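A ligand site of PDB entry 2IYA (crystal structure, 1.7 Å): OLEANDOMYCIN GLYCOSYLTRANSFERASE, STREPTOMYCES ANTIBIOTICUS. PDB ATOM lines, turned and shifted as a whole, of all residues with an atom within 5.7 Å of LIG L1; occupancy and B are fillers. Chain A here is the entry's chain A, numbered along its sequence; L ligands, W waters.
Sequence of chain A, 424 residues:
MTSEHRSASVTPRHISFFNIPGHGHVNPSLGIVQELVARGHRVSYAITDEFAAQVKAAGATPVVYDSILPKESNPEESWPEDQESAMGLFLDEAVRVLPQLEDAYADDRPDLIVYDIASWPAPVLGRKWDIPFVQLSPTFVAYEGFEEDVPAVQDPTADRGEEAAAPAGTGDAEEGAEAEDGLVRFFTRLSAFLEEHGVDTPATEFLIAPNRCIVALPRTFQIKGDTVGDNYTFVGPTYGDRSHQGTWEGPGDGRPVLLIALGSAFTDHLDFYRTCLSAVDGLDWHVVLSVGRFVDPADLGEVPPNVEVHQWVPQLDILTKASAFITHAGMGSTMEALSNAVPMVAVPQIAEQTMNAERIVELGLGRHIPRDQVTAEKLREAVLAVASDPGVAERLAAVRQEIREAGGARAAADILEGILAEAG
Water W7 lies within hydrogen-bond range of O of Gly 24 (2.6 Å), O7 of LIG L1 (2.8 Å) and N of Gly 332 (3.2 Å).
Water W9 lies within hydrogen-bond range of an oxygen (O11) of LIG L1 (2.9 Å) and the side-chain amide nitrogen of Gln 353 (3.1 Å).
Water W8 lies within hydrogen-bond range of ND2 of Asn 27, O1 of LIG L1 and NE2 of Gln 245.
Water W3 lies within hydrogen-bond range of the backbone carbonyl oxygen of Gln 311 (2.8 Å), the side-chain hydroxyl of Ser 290 (3.1 Å) and an oxygen (O2) of LIG L1 (3.4 Å).
Water W11 lies within hydrogen-bond range of the backbone NH of Met 331 (2.9 Å) and an oxygen (O7) of LIG L1 (3.4 Å).
Water W1 lies within hydrogen-bond range of the side-chain amide oxygen of Gln 315 (2.6 Å), the backbone NH of Gly 263 (2.9 Å) and the side-chain hydroxyl of Ser 333 (3.0 Å).
An oxygen (O5) of LIG L1 lies within hydrogen-bond range of the side-chain carboxylate (OE2) of Glu 336 (2.6 Å).
N of Ser 264 is in hydrogen-bond range of O10 of LIG L1, at 2.8 Å.
The side-chain hydroxyl (OG) of Ser 264 lies within hydrogen-bond range of an oxygen (O10) of LIG L1 (2.7 Å).
The backbone NH (N) of Ser 333 sits at hydrogen-bond distance from an oxygen (O8) of LIG L1.
The side-chain hydroxyl (OG) of Ser 333 is in hydrogen-bond range of an oxygen (O8) of LIG L1 (2.7 Å).
N of Val 313 is in hydrogen-bond range of O2 of LIG L1 (3.0 Å).
The backbone carbonyl oxygen of Val 313 is in hydrogen-bond range of a nitrogen (N2) of LIG L1, at 2.7 Å.
NE2 of His 328 is in hydrogen-bond range of O11 of LIG L1 (2.9 Å).
The side-chain hydroxyl of Ser 290 is in hydrogen-bond range of an oxygen (O2) of LIG L1, at 2.9 Å.
The backbone NH (N) of Gly 332 sits at hydrogen-bond distance from an oxygen (O7) of LIG L1.
The side-chain amide nitrogen of Asn 27 sits at hydrogen-bond distance from an oxygen (O5) of LIG L1 (3.1 Å).
O1 of LIG L1 lies within hydrogen-bond range of NE2 of Gln 245, at 3.1 Å.
An oxygen (O3) of LIG L1 is in hydrogen-bond range of the side-chain amide nitrogen (NE2) of Gln 315 (3.2 Å).
The guanidinium group (NH1) of Arg 242 sits at hydrogen-bond distance from an oxygen (O3) of LIG L1, at 3.4 Å.
O8 of LG2 L2 sits at hydrogen-bond distance from NE2 of His 25 (2.7 Å).
NE2 of Gln 315 sits at hydrogen-bond distance from OE1 of Glu 336, at 2.9 Å.
The side-chain carboxylate (OE2) of Glu 336 lies within salt-bridge range of the guanidinium group (NH1) of Arg 242 (2.9 Å).
OG of Ser 333 lies within hydrogen-bond range of NE2 of Gln 315.
ND1 of His 328 sits close to N of Gly 330 (3.4 Å).
The side-chain hydroxyl (OG) of Ser 290 lies within hydrogen-bond range of the backbone carbonyl oxygen (O) of Gln 311 (3.3 Å).
NE1 of Trp 312 lies close to NE2 of Gln 245, at 3.3 Å.
OG1 of Thr 334 sits at hydrogen-bond distance from O of Gly 330, at 2.9 Å.
His 23 touches LIG L1 (CB to O4, 3.9 Å).
Gly 24 touches LIG L1.
Gly 263 touches LIG L1 (O to C3, 3.7 Å).
Ala 265 touches LIG L1 (N to O10, 3.9 Å).
Trp 312 touches LIG L1.
Gly 330 touches LIG L1 (CA to O8, 3.6 Å).
Met 331 touches LIG L1.
NE2 of Gln 353 touches O11 of LIG L1, 3.8 Å away.
Hydrophobic or aromatic side chains within 4 Å of LIG L1: His 23, Trp 312, Val 313 and His 328.
The nearest printed residue that does not touch LIG L1 is Leu 316 (4.5 Å).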
ATOM      1  N   HIS A  23      13.454  24.447 -16.859  1.00  0.00           N
ATOM      2  CA  HIS A  23      13.572  25.201 -15.601  1.00  0.00           C
ATOM      3  C   HIS A  23      13.035  24.422 -14.405  1.00  0.00           C
ATOM      4  O   HIS A  23      13.584  24.527 -13.300  1.00  0.00           O
ATOM      5  CB  HIS A  23      12.875  26.578 -15.649  1.00  0.00           C
ATOM      6  CG  HIS A  23      13.597  27.595 -16.466  1.00  0.00           C
ATOM      7  ND1 HIS A  23      14.543  28.456 -15.945  1.00  0.00           N
ATOM      8  CD2 HIS A  23      13.514  27.901 -17.783  1.00  0.00           C
ATOM      9  CE1 HIS A  23      15.013  29.233 -16.899  1.00  0.00           C
ATOM     10  NE2 HIS A  23      14.406  28.918 -18.021  1.00  0.00           N
ATOM     11  N   GLY A  24      11.985  23.635 -14.626  1.00  0.00           N
ATOM     12  CA  GLY A  24      11.426  22.827 -13.553  1.00  0.00           C
ATOM     13  C   GLY A  24      12.340  21.711 -13.044  1.00  0.00           C
ATOM     14  O   GLY A  24      12.231  21.259 -11.897  1.00  0.00           O
ATOM     15  N   HIS A  25      13.277  21.287 -13.900  1.00  0.00           N
ATOM     16  CA  HIS A  25      14.278  20.290 -13.493  1.00  0.00           C
ATOM     17  C   HIS A  25      15.565  20.961 -12.974  1.00  0.00           C
ATOM     18  O   HIS A  25      16.143  20.496 -12.011  1.00  0.00           O
ATOM     19  CB  HIS A  25      14.573  19.337 -14.635  1.00  0.00           C
ATOM     20  CG  HIS A  25      13.421  18.450 -14.974  1.00  0.00           C
ATOM     21  ND1 HIS A  25      13.440  17.085 -14.753  1.00  0.00           N
ATOM     22  CD2 HIS A  25      12.191  18.729 -15.451  1.00  0.00           C
ATOM     23  CE1 HIS A  25      12.286  16.562 -15.120  1.00  0.00           C
ATOM     24  NE2 HIS A  25      11.495  17.550 -15.532  1.00  0.00           N
ATOM     25  N   ASN A  27      16.012  24.284 -11.707  1.00  0.00           N
ATOM     26  CA  ASN A  27      15.898  25.197 -10.561  1.00  0.00           C
ATOM     27  C   ASN A  27      16.094  24.575  -9.183  1.00  0.00           C
ATOM     28  O   ASN A  27      16.845  25.139  -8.374  1.00  0.00           O
ATOM     29  CB  ASN A  27      14.613  26.042 -10.616  1.00  0.00           C
ATOM     30  CG  ASN A  27      14.712  27.162 -11.594  1.00  0.00           C
ATOM     31  OD1 ASN A  27      15.792  27.383 -12.145  1.00  0.00           O
ATOM     32  ND2 ASN A  27      13.615  27.881 -11.823  1.00  0.00           N
ATOM     33  N   ARG A 242      17.985  33.240  -5.817  1.00  0.00           N
ATOM     34  CA  ARG A 242      17.750  33.435  -7.252  1.00  0.00           C
ATOM     35  C   ARG A 242      17.996  34.888  -7.681  1.00  0.00           C
ATOM     36  O   ARG A 242      17.280  35.422  -8.525  1.00  0.00           O
ATOM     37  CB  ARG A 242      16.325  32.990  -7.607  1.00  0.00           C
ATOM     38  CG  ARG A 242      16.154  32.461  -9.016  1.00  0.00           C
ATOM     39  CD  ARG A 242      14.875  31.633  -9.117  1.00  0.00           C
ATOM     40  NE  ARG A 242      15.000  30.264  -8.606  1.00  0.00           N
ATOM     41  CZ  ARG A 242      13.956  29.442  -8.429  1.00  0.00           C
ATOM     42  NH1 ARG A 242      12.719  29.855  -8.713  1.00  0.00           N
ATOM     43  NH2 ARG A 242      14.129  28.218  -7.967  1.00  0.00           N
ATOM     44  N   GLN A 245      17.959  36.282 -11.323  1.00  0.00           N
ATOM     45  CA  GLN A 245      16.716  36.774 -11.941  1.00  0.00           C
ATOM     46  C   GLN A 245      16.416  38.240 -11.607  1.00  0.00           C
ATOM     47  O   GLN A 245      15.552  38.873 -12.219  1.00  0.00           O
ATOM     48  CB  GLN A 245      15.527  35.920 -11.514  1.00  0.00           C
ATOM     49  CG  GLN A 245      15.379  34.621 -12.267  1.00  0.00           C
ATOM     50  CD  GLN A 245      13.963  34.056 -12.172  1.00  0.00           C
ATOM     51  OE1 GLN A 245      13.392  33.959 -11.076  1.00  0.00           O
ATOM     52  NE2 GLN A 245      13.375  33.713 -13.316  1.00  0.00           N
ATOM     53  N   ALA A 261       0.866  32.428 -13.473  1.00  0.00           N
ATOM     54  CA  ALA A 261       1.945  31.818 -14.258  1.00  0.00           C
ATOM     55  C   ALA A 261       1.730  30.308 -14.336  1.00  0.00           C
ATOM     56  O   ALA A 261       1.561  29.654 -13.296  1.00  0.00           O
ATOM     57  CB  ALA A 261       3.295  32.129 -13.652  1.00  0.00           C
ATOM     58  N   LEU A 262       1.782  29.772 -15.549  1.00  0.00           N
ATOM     59  CA  LEU A 262       1.604  28.328 -15.802  1.00  0.00           C
ATOM     60  C   LEU A 262       2.933  27.550 -16.044  1.00  0.00           C
ATOM     61  O   LEU A 262       2.994  26.543 -16.806  1.00  0.00           O
ATOM     62  CB  LEU A 262       0.635  28.126 -16.968  1.00  0.00           C
ATOM     63  CG  LEU A 262      -0.728  28.834 -16.953  1.00  0.00           C
ATOM     64  CD1 LEU A 262      -1.469  28.515 -18.263  1.00  0.00           C
ATOM     65  CD2 LEU A 262      -1.586  28.443 -15.727  1.00  0.00           C
ATOM     66  N   GLY A 263       4.003  27.967 -15.384  1.00  0.00           N
ATOM     67  CA  GLY A 263       5.245  27.195 -15.473  1.00  0.00           C
ATOM     68  C   GLY A 263       6.133  27.560 -16.641  1.00  0.00           C
ATOM     69  O   GLY A 263       5.979  28.625 -17.228  1.00  0.00           O
ATOM     70  N   SER A 264       7.072  26.668 -16.966  1.00  0.00           N
ATOM     71  CA  SER A 264       8.053  26.982 -18.000  1.00  0.00           C
ATOM     72  C   SER A 264       7.845  26.180 -19.281  1.00  0.00           C
ATOM     73  O   SER A 264       8.618  26.315 -20.226  1.00  0.00           O
ATOM     74  CB  SER A 264       9.493  26.821 -17.497  1.00  0.00           C
ATOM     75  OG  SER A 264       9.734  25.465 -17.138  1.00  0.00           O
ATOM     76  N   ALA A 265       6.797  25.358 -19.325  1.00  0.00           N
ATOM     77  CA  ALA A 265       6.621  24.475 -20.483  1.00  0.00           C
ATOM     78  C   ALA A 265       5.259  24.571 -21.164  1.00  0.00           C
ATOM     79  O   ALA A 265       5.198  24.838 -22.375  1.00  0.00           O
ATOM     80  CB  ALA A 265       6.944  23.008 -20.115  1.00  0.00           C
ATOM     81  N   PHE A 266       4.202  24.363 -20.421  1.00  0.00           N
ATOM     82  CA  PHE A 266       2.882  24.174 -21.058  1.00  0.00           C
ATOM     83  C   PHE A 266       2.059  25.458 -20.951  1.00  0.00           C
ATOM     84  O   PHE A 266       1.019  25.489 -20.308  1.00  0.00           O
ATOM     85  CB  PHE A 266       2.158  23.001 -20.405  1.00  0.00           C
ATOM     86  CG  PHE A 266       2.840  21.689 -20.652  1.00  0.00           C
ATOM     87  CD1 PHE A 266       2.781  21.096 -21.907  1.00  0.00           C
ATOM     88  CD2 PHE A 266       3.589  21.071 -19.645  1.00  0.00           C
ATOM     89  CE1 PHE A 266       3.432  19.865 -22.157  1.00  0.00           C
ATOM     90  CE2 PHE A 266       4.230  19.869 -19.882  1.00  0.00           C
ATOM     91  CZ  PHE A 266       4.152  19.275 -21.127  1.00  0.00           C
ATOM     92  N   SER A 290       2.222  36.263 -16.293  1.00  0.00           N
ATOM     93  CA  SER A 290       3.331  35.723 -17.093  1.00  0.00           C
ATOM     94  C   SER A 290       2.697  34.841 -18.153  1.00  0.00           C
ATOM     95  O   SER A 290       1.947  33.913 -17.779  1.00  0.00           O
ATOM     96  CB  SER A 290       4.260  34.915 -16.206  1.00  0.00           C
ATOM     97  OG  SER A 290       5.369  34.451 -16.948  1.00  0.00           O
ATOM     98  N   GLN A 311       6.390  37.834 -20.806  1.00  0.00           N
ATOM     99  CA  GLN A 311       6.520  36.408 -21.144  1.00  0.00           C
ATOM    100  C   GLN A 311       7.133  35.607 -20.000  1.00  0.00           C
ATOM    101  O   GLN A 311       6.880  34.412 -19.889  1.00  0.00           O
ATOM    102  CB  GLN A 311       7.380  36.188 -22.383  1.00  0.00           C
ATOM    103  CG  GLN A 311       6.697  36.640 -23.667  1.00  0.00           C
ATOM    104  CD  GLN A 311       7.388  36.097 -24.901  1.00  0.00           C
ATOM    105  OE1 GLN A 311       8.599  35.910 -24.908  1.00  0.00           O
ATOM    106  NE2 GLN A 311       6.621  35.866 -25.952  1.00  0.00           N
ATOM    107  N   TRP A 312       7.974  36.251 -19.195  1.00  0.00           N
ATOM    108  CA  TRP A 312       8.755  35.540 -18.156  1.00  0.00           C
ATOM    109  C   TRP A 312       9.011  36.503 -16.992  1.00  0.00           C
ATOM    110  O   TRP A 312       9.322  37.680 -17.236  1.00  0.00           O
ATOM    111  CB  TRP A 312      10.047  35.024 -18.756  1.00  0.00           C
ATOM    112  CG  TRP A 312      10.986  34.313 -17.830  1.00  0.00           C
ATOM    113  CD1 TRP A 312      12.113  34.819 -17.264  1.00  0.00           C
ATOM    114  CD2 TRP A 312      10.909  32.932 -17.418  1.00  0.00           C
ATOM    115  NE1 TRP A 312      12.750  33.850 -16.506  1.00  0.00           N
ATOM    116  CE2 TRP A 312      12.014  32.690 -16.575  1.00  0.00           C
ATOM    117  CE3 TRP A 312      10.008  31.897 -17.674  1.00  0.00           C
ATOM    118  CZ2 TRP A 312      12.259  31.435 -15.986  1.00  0.00           C
ATOM    119  CZ3 TRP A 312      10.244  30.642 -17.085  1.00  0.00           C
ATOM    120  CH2 TRP A 312      11.359  30.432 -16.259  1.00  0.00           C
ATOM    121  N   VAL A 313       8.823  36.044 -15.764  1.00  0.00           N
ATOM    122  CA  VAL A 313       8.970  36.904 -14.587  1.00  0.00           C
ATOM    123  C   VAL A 313       9.871  36.300 -13.501  1.00  0.00           C
ATOM    124  O   VAL A 313      10.125  35.098 -13.530  1.00  0.00           O
ATOM    125  CB  VAL A 313       7.588  37.278 -13.968  1.00  0.00           C
ATOM    126  CG1 VAL A 313       6.698  37.969 -15.007  1.00  0.00           C
ATOM    127  CG2 VAL A 313       6.894  36.049 -13.361  1.00  0.00           C
ATOM    128  N   PRO A 314      10.353  37.132 -12.553  1.00  0.00           N
ATOM    129  CA  PRO A 314      11.075  36.600 -11.387  1.00  0.00           C
ATOM    130  C   PRO A 314      10.054  36.049 -10.404  1.00  0.00           C
ATOM    131  O   PRO A 314       9.688  36.694  -9.407  1.00  0.00           O
ATOM    132  CB  PRO A 314      11.771  37.843 -10.778  1.00  0.00           C
ATOM    133  CG  PRO A 314      11.224  39.016 -11.459  1.00  0.00           C
ATOM    134  CD  PRO A 314      10.258  38.605 -12.533  1.00  0.00           C
ATOM    135  N   GLN A 315       9.604  34.840 -10.712  1.00  0.00           N
ATOM    136  CA  GLN A 315       8.479  34.249  -9.952  1.00  0.00           C
ATOM    137  C   GLN A 315       8.755  34.110  -8.473  1.00  0.00           C
ATOM    138  O   GLN A 315       7.877  34.408  -7.658  1.00  0.00           O
ATOM    139  CB  GLN A 315       8.105  32.895 -10.556  1.00  0.00           C
ATOM    140  CG  GLN A 315       7.163  32.081  -9.657  1.00  0.00           C
ATOM    141  CD  GLN A 315       6.586  30.896 -10.353  1.00  0.00           C
ATOM    142  OE1 GLN A 315       6.136  31.014 -11.489  1.00  0.00           O
ATOM    143  NE2 GLN A 315       6.592  29.734  -9.692  1.00  0.00           N
ATOM    144  N   LEU A 316       9.943  33.620  -8.114  1.00  0.00           N
ATOM    145  CA  LEU A 316      10.218  33.387  -6.704  1.00  0.00           C
ATOM    146  C   LEU A 316      10.165  34.717  -5.964  1.00  0.00           C
ATOM    147  O   LEU A 316       9.522  34.833  -4.899  1.00  0.00           O
ATOM    148  CB  LEU A 316      11.574  32.690  -6.507  1.00  0.00           C
ATOM    149  CG  LEU A 316      11.960  32.433  -5.051  1.00  0.00           C
ATOM    150  CD1 LEU A 316      10.917  31.590  -4.283  1.00  0.00           C
ATOM    151  CD2 LEU A 316      13.344  31.783  -5.031  1.00  0.00           C
ATOM    152  N   HIS A 328      -0.294  26.328 -12.622  1.00  0.00           N
ATOM    153  CA  HIS A 328      -0.588  25.000 -13.174  1.00  0.00           C
ATOM    154  C   HIS A 328      -0.316  23.886 -12.132  1.00  0.00           C
ATOM    155  O   HIS A 328      -0.615  22.733 -12.389  1.00  0.00           O
ATOM    156  CB  HIS A 328       0.221  24.762 -14.444  1.00  0.00           C
ATOM    157  CG  HIS A 328       1.686  24.575 -14.215  1.00  0.00           C
ATOM    158  ND1 HIS A 328       2.419  25.331 -13.308  1.00  0.00           N
ATOM    159  CD2 HIS A 328       2.580  23.735 -14.796  1.00  0.00           C
ATOM    160  CE1 HIS A 328       3.680  24.944 -13.324  1.00  0.00           C
ATOM    161  NE2 HIS A 328       3.799  23.969 -14.214  1.00  0.00           N
ATOM    162  N   ALA A 329       0.252  24.258 -10.975  1.00  0.00           N
ATOM    163  CA  ALA A 329       0.594  23.292  -9.911  1.00  0.00           C
ATOM    164  C   ALA A 329       1.722  22.335 -10.295  1.00  0.00           C
ATOM    165  O   ALA A 329       1.755  21.200  -9.823  1.00  0.00           O
ATOM    166  CB  ALA A 329      -0.664  22.501  -9.396  1.00  0.00           C
ATOM    167  N   GLY A 330       2.666  22.802 -11.124  1.00  0.00           N
ATOM    168  CA  GLY A 330       3.957  22.113 -11.247  1.00  0.00           C
ATOM    169  C   GLY A 330       4.572  22.042  -9.838  1.00  0.00           C
ATOM    170  O   GLY A 330       4.292  22.911  -9.004  1.00  0.00           O
ATOM    171  N   MET A 331       5.430  21.057  -9.568  1.00  0.00           N
ATOM    172  CA  MET A 331       5.944  20.927  -8.183  1.00  0.00           C
ATOM    173  C   MET A 331       6.797  22.103  -7.723  1.00  0.00           C
ATOM    174  O   MET A 331       6.726  22.512  -6.551  1.00  0.00           O
ATOM    175  CB  MET A 331       6.723  19.618  -7.999  1.00  0.00           C
ATOM    176  CG  MET A 331       7.010  19.306  -6.495  1.00  0.00           C
ATOM    177  SD  MET A 331       5.539  18.959  -5.446  1.00  0.00           S
ATOM    178  CE  MET A 331       5.145  17.307  -6.076  1.00  0.00           C
ATOM    179  N   GLY A 332       7.640  22.615  -8.616  1.00  0.00           N
ATOM    180  CA  GLY A 332       8.501  23.763  -8.280  1.00  0.00           C
ATOM    181  C   GLY A 332       7.653  24.969  -7.868  1.00  0.00           C
ATOM    182  O   GLY A 332       7.898  25.611  -6.822  1.00  0.00           O
ATOM    183  N   SER A 333       6.677  25.292  -8.717  1.00  0.00           N
ATOM    184  CA  SER A 333       5.797  26.431  -8.451  1.00  0.00           C
ATOM    185  C   SER A 333       5.020  26.233  -7.130  1.00  0.00           C
ATOM    186  O   SER A 333       4.890  27.166  -6.333  1.00  0.00           O
ATOM    187  CB  SER A 333       4.866  26.682  -9.628  1.00  0.00           C
ATOM    188  OG  SER A 333       5.625  27.094 -10.759  1.00  0.00           O
ATOM    189  N   THR A 334       4.548  25.009  -6.928  1.00  0.00           N
ATOM    190  CA  THR A 334       3.831  24.619  -5.704  1.00  0.00           C
ATOM    191  C   THR A 334       4.720  24.837  -4.496  1.00  0.00           C
ATOM    192  O   THR A 334       4.324  25.505  -3.547  1.00  0.00           O
ATOM    193  CB  THR A 334       3.345  23.170  -5.793  1.00  0.00           C
ATOM    194  OG1 THR A 334       2.377  23.079  -6.848  1.00  0.00           O
ATOM    195  CG2 THR A 334       2.670  22.729  -4.444  1.00  0.00           C
ATOM    196  N   GLU A 336       7.478  26.657  -4.224  1.00  0.00           N
ATOM    197  CA  GLU A 336       7.825  28.087  -4.034  1.00  0.00           C
ATOM    198  C   GLU A 336       6.683  28.878  -3.353  1.00  0.00           C
ATOM    199  O   GLU A 336       6.905  29.701  -2.431  1.00  0.00           O
ATOM    200  CB  GLU A 336       8.230  28.735  -5.350  1.00  0.00           C
ATOM    201  CG  GLU A 336       9.543  28.148  -5.936  1.00  0.00           C
ATOM    202  CD  GLU A 336       9.727  28.419  -7.421  1.00  0.00           C
ATOM    203  OE1 GLU A 336       8.883  29.112  -8.029  1.00  0.00           O
ATOM    204  OE2 GLU A 336      10.729  27.910  -7.995  1.00  0.00           O
ATOM    205  N   GLN A 353       0.461  17.310 -12.792  1.00  0.00           N
ATOM    206  CA  GLN A 353      -0.064  18.540 -12.183  1.00  0.00           C
ATOM    207  C   GLN A 353      -1.443  18.342 -11.564  1.00  0.00           C
ATOM    208  O   GLN A 353      -1.738  18.923 -10.534  1.00  0.00           O
ATOM    209  CB  GLN A 353      -0.066  19.662 -13.189  1.00  0.00           C
ATOM    210  CG  GLN A 353       1.367  20.114 -13.485  1.00  0.00           C
ATOM    211  CD  GLN A 353       1.551  20.540 -14.907  1.00  0.00           C
ATOM    212  OE1 GLN A 353       0.598  20.773 -15.643  1.00  0.00           O
ATOM    213  NE2 GLN A 353       2.814  20.620 -15.324  1.00  0.00           N
HETATM  214  N1  LIG L   1       9.355  30.308 -13.525  1.00  0.00           N
HETATM  215  C1  LIG L   1       9.911  31.580 -13.473  1.00  0.00           C
HETATM  216  N2  LIG L   1       9.295  32.612 -14.165  1.00  0.00           N
HETATM  217  C2  LIG L   1       8.133  32.400 -14.876  1.00  0.00           C
HETATM  218  C3  LIG L   1       7.558  31.118 -14.928  1.00  0.00           C
HETATM  219  C4  LIG L   1       8.184  30.095 -14.226  1.00  0.00           C
HETATM  220  O1  LIG L   1      10.940  31.810 -12.858  1.00  0.00           O
HETATM  221  O2  LIG L   1       7.629  33.354 -15.467  1.00  0.00           O
HETATM  222  C5  LIG L   1      10.023  29.220 -12.778  1.00  0.00           C
HETATM  223  C6  LIG L   1       9.316  28.922 -11.456  1.00  0.00           C
HETATM  224  O3  LIG L   1       9.740  29.808 -10.443  1.00  0.00           O
HETATM  225  C7  LIG L   1       9.666  27.456 -11.209  1.00  0.00           C
HETATM  226  C8  LIG L   1       9.845  26.898 -12.627  1.00  0.00           C
HETATM  227  O4  LIG L   1       9.985  28.010 -13.516  1.00  0.00           O
HETATM  228  O5  LIG L   1      10.899  27.308 -10.521  1.00  0.00           O
HETATM  229  C9  LIG L   1       8.679  26.057 -13.152  1.00  0.00           C
HETATM  230  O6  LIG L   1       8.784  24.772 -12.574  1.00  0.00           O
HETATM  231  P1  LIG L   1       7.493  23.898 -12.256  1.00  0.00           P
HETATM  232  O7  LIG L   1       7.970  22.711 -11.535  1.00  0.00           O
HETATM  233  O8  LIG L   1       6.443  24.642 -11.510  1.00  0.00           O
HETATM  234  O9  LIG L   1       6.691  23.663 -13.618  1.00  0.00           O
HETATM  235  P2  LIG L   1       7.169  23.136 -15.038  1.00  0.00           P
HETATM  236  O10 LIG L   1       7.833  24.271 -15.713  1.00  0.00           O
HETATM  237  O11 LIG L   1       5.950  22.699 -15.698  1.00  0.00           O
HETATM  238  O12 LIG L   1       8.118  22.016 -14.821  1.00  0.00           O
HETATM  239  C1  LG2 L   2      10.166   8.388 -15.377  1.00  0.00           C
HETATM  240  C2  LG2 L   2       9.195   8.522 -14.184  1.00  0.00           C
HETATM  241  C3  LG2 L   2       9.661   8.244 -12.720  1.00  0.00           C
HETATM  242  C4  LG2 L   2       8.486   8.507 -11.743  1.00  0.00           C
HETATM  243  O1  LG2 L   2       8.179   9.898 -11.817  1.00  0.00           O
HETATM  244  C5  LG2 L   2       6.925  11.865 -12.768  1.00  0.00           C
HETATM  245  C6  LG2 L   2       6.768  12.059 -14.304  1.00  0.00           C
HETATM  246  C7  LG2 L   2       7.543  13.296 -14.882  1.00  0.00           C
HETATM  247  C8  LG2 L   2       7.566  13.343 -16.444  1.00  0.00           C
HETATM  248  C9  LG2 L   2       8.140  12.061 -17.149  1.00  0.00           C
HETATM  249  C10 LG2 L   2       9.665  12.051 -16.875  1.00  0.00           C
HETATM  250  C11 LG2 L   2      10.444  10.748 -16.641  1.00  0.00           C
HETATM  251  C12 LG2 L   2       9.733   9.405 -16.455  1.00  0.00           C
HETATM  252  O2  LG2 L   2       8.651   9.051 -17.271  1.00  0.00           O
HETATM  253  C13 LG2 L   2       7.036  10.355 -12.490  1.00  0.00           C
HETATM  254  O3  LG2 L   2       6.081   9.453 -12.994  1.00  0.00           O
HETATM  255  O4  LG2 L   2       5.401  12.127 -14.666  1.00  0.00           O
HETATM  256  O5  LG2 L   2       8.415  14.423 -16.836  1.00  0.00           O
HETATM  257  C14 LG2 L   2      10.362   6.984 -15.965  1.00  0.00           C
HETATM  258  C15 LG2 L   2      11.680  10.630 -17.546  1.00  0.00           C
HETATM  259  C16 LG2 L   2      10.875   9.094 -12.296  1.00  0.00           C
HETATM  260  O6  LG2 L   2       7.972   7.863 -14.492  1.00  0.00           O
HETATM  261  C17 LG2 L   2       8.773   8.158 -10.273  1.00  0.00           C
HETATM  262  C18 LG2 L   2       5.807  12.436 -11.875  1.00  0.00           C
HETATM  263  C19 LG2 L   2       7.874  11.992 -18.666  1.00  0.00           C
HETATM  264  C20 LG2 L   2       7.700  15.480 -17.464  1.00  0.00           C
HETATM  265  C21 LG2 L   2       8.635  16.698 -17.474  1.00  0.00           C
HETATM  266  C22 LG2 L   2       8.036  17.845 -18.317  1.00  0.00           C
HETATM  267  C23 LG2 L   2       7.565  17.352 -19.698  1.00  0.00           C
HETATM  268  C24 LG2 L   2       6.623  16.158 -19.505  1.00  0.00           C
HETATM  269  O7  LG2 L   2       7.299  15.133 -18.783  1.00  0.00           O
HETATM  270  N1  LG2 L   2       8.920  19.015 -18.361  1.00  0.00           N
HETATM  271  C25 LG2 L   2       6.193  15.520 -20.828  1.00  0.00           C
HETATM  272  O8  LG2 L   2       8.876  17.156 -16.153  1.00  0.00           O
HETATM  273  C26 LG2 L   2       8.275  20.200 -18.959  1.00  0.00           C
HETATM  274  C27 LG2 L   2       4.870  11.171 -15.574  1.00  0.00           C
HETATM  275  C28 LG2 L   2       3.511  10.697 -15.010  1.00  0.00           C
HETATM  276  C29 LG2 L   2       2.425  11.814 -15.084  1.00  0.00           C
HETATM  277  C30 LG2 L   2       2.388  12.412 -16.517  1.00  0.00           C
HETATM  278  C31 LG2 L   2       3.819  12.787 -16.980  1.00  0.00           C
HETATM  279  O9  LG2 L   2       4.735  11.698 -16.891  1.00  0.00           O
HETATM  280  O10 LG2 L   2       1.123  11.319 -14.733  1.00  0.00           O
HETATM  281  O11 LG2 L   2       1.613  13.604 -16.519  1.00  0.00           O
HETATM  282  O12 LG2 L   2      11.772  10.839 -16.154  1.00  0.00           O
HETATM  283  C32 LG2 L   2       1.008  11.075 -13.327  1.00  0.00           C
HETATM  284  C33 LG2 L   2      10.314  18.816 -18.794  1.00  0.00           C
HETATM  285  C34 LG2 L   2       3.862  13.286 -18.433  1.00  0.00           C
HETATM  286  C35 LG2 L   2       7.059  14.613 -14.226  1.00  0.00           C
HETATM  287  O   HOH W   1       5.150  29.061 -12.948  1.00  0.00           O
HETATM  288  O   HOH W   2       4.770  24.447 -17.583  1.00  0.00           O
HETATM  289  O   HOH W   3       6.745  32.055 -18.427  1.00  0.00           O
HETATM  290  O   HOH W   4       9.254  19.878 -13.191  1.00  0.00           O
HETATM  291  O   HOH W   5      11.633  24.654  -9.762  1.00  0.00           O
HETATM  292  O   HOH W   6      11.626  32.247 -10.041  1.00  0.00           O
HETATM  293  O   HOH W   7      10.405  22.204 -10.256  1.00  0.00           O
HETATM  294  O   HOH W   8      13.574  30.525 -13.006  1.00  0.00           O
HETATM  295  O   HOH W   9       5.441  20.078 -16.852  1.00  0.00           O
HETATM  296  O   HOH W  10       5.150  19.918 -14.000  1.00  0.00           O
HETATM  297  O   HOH W  11       6.529  19.586 -11.764  1.00  0.00           O
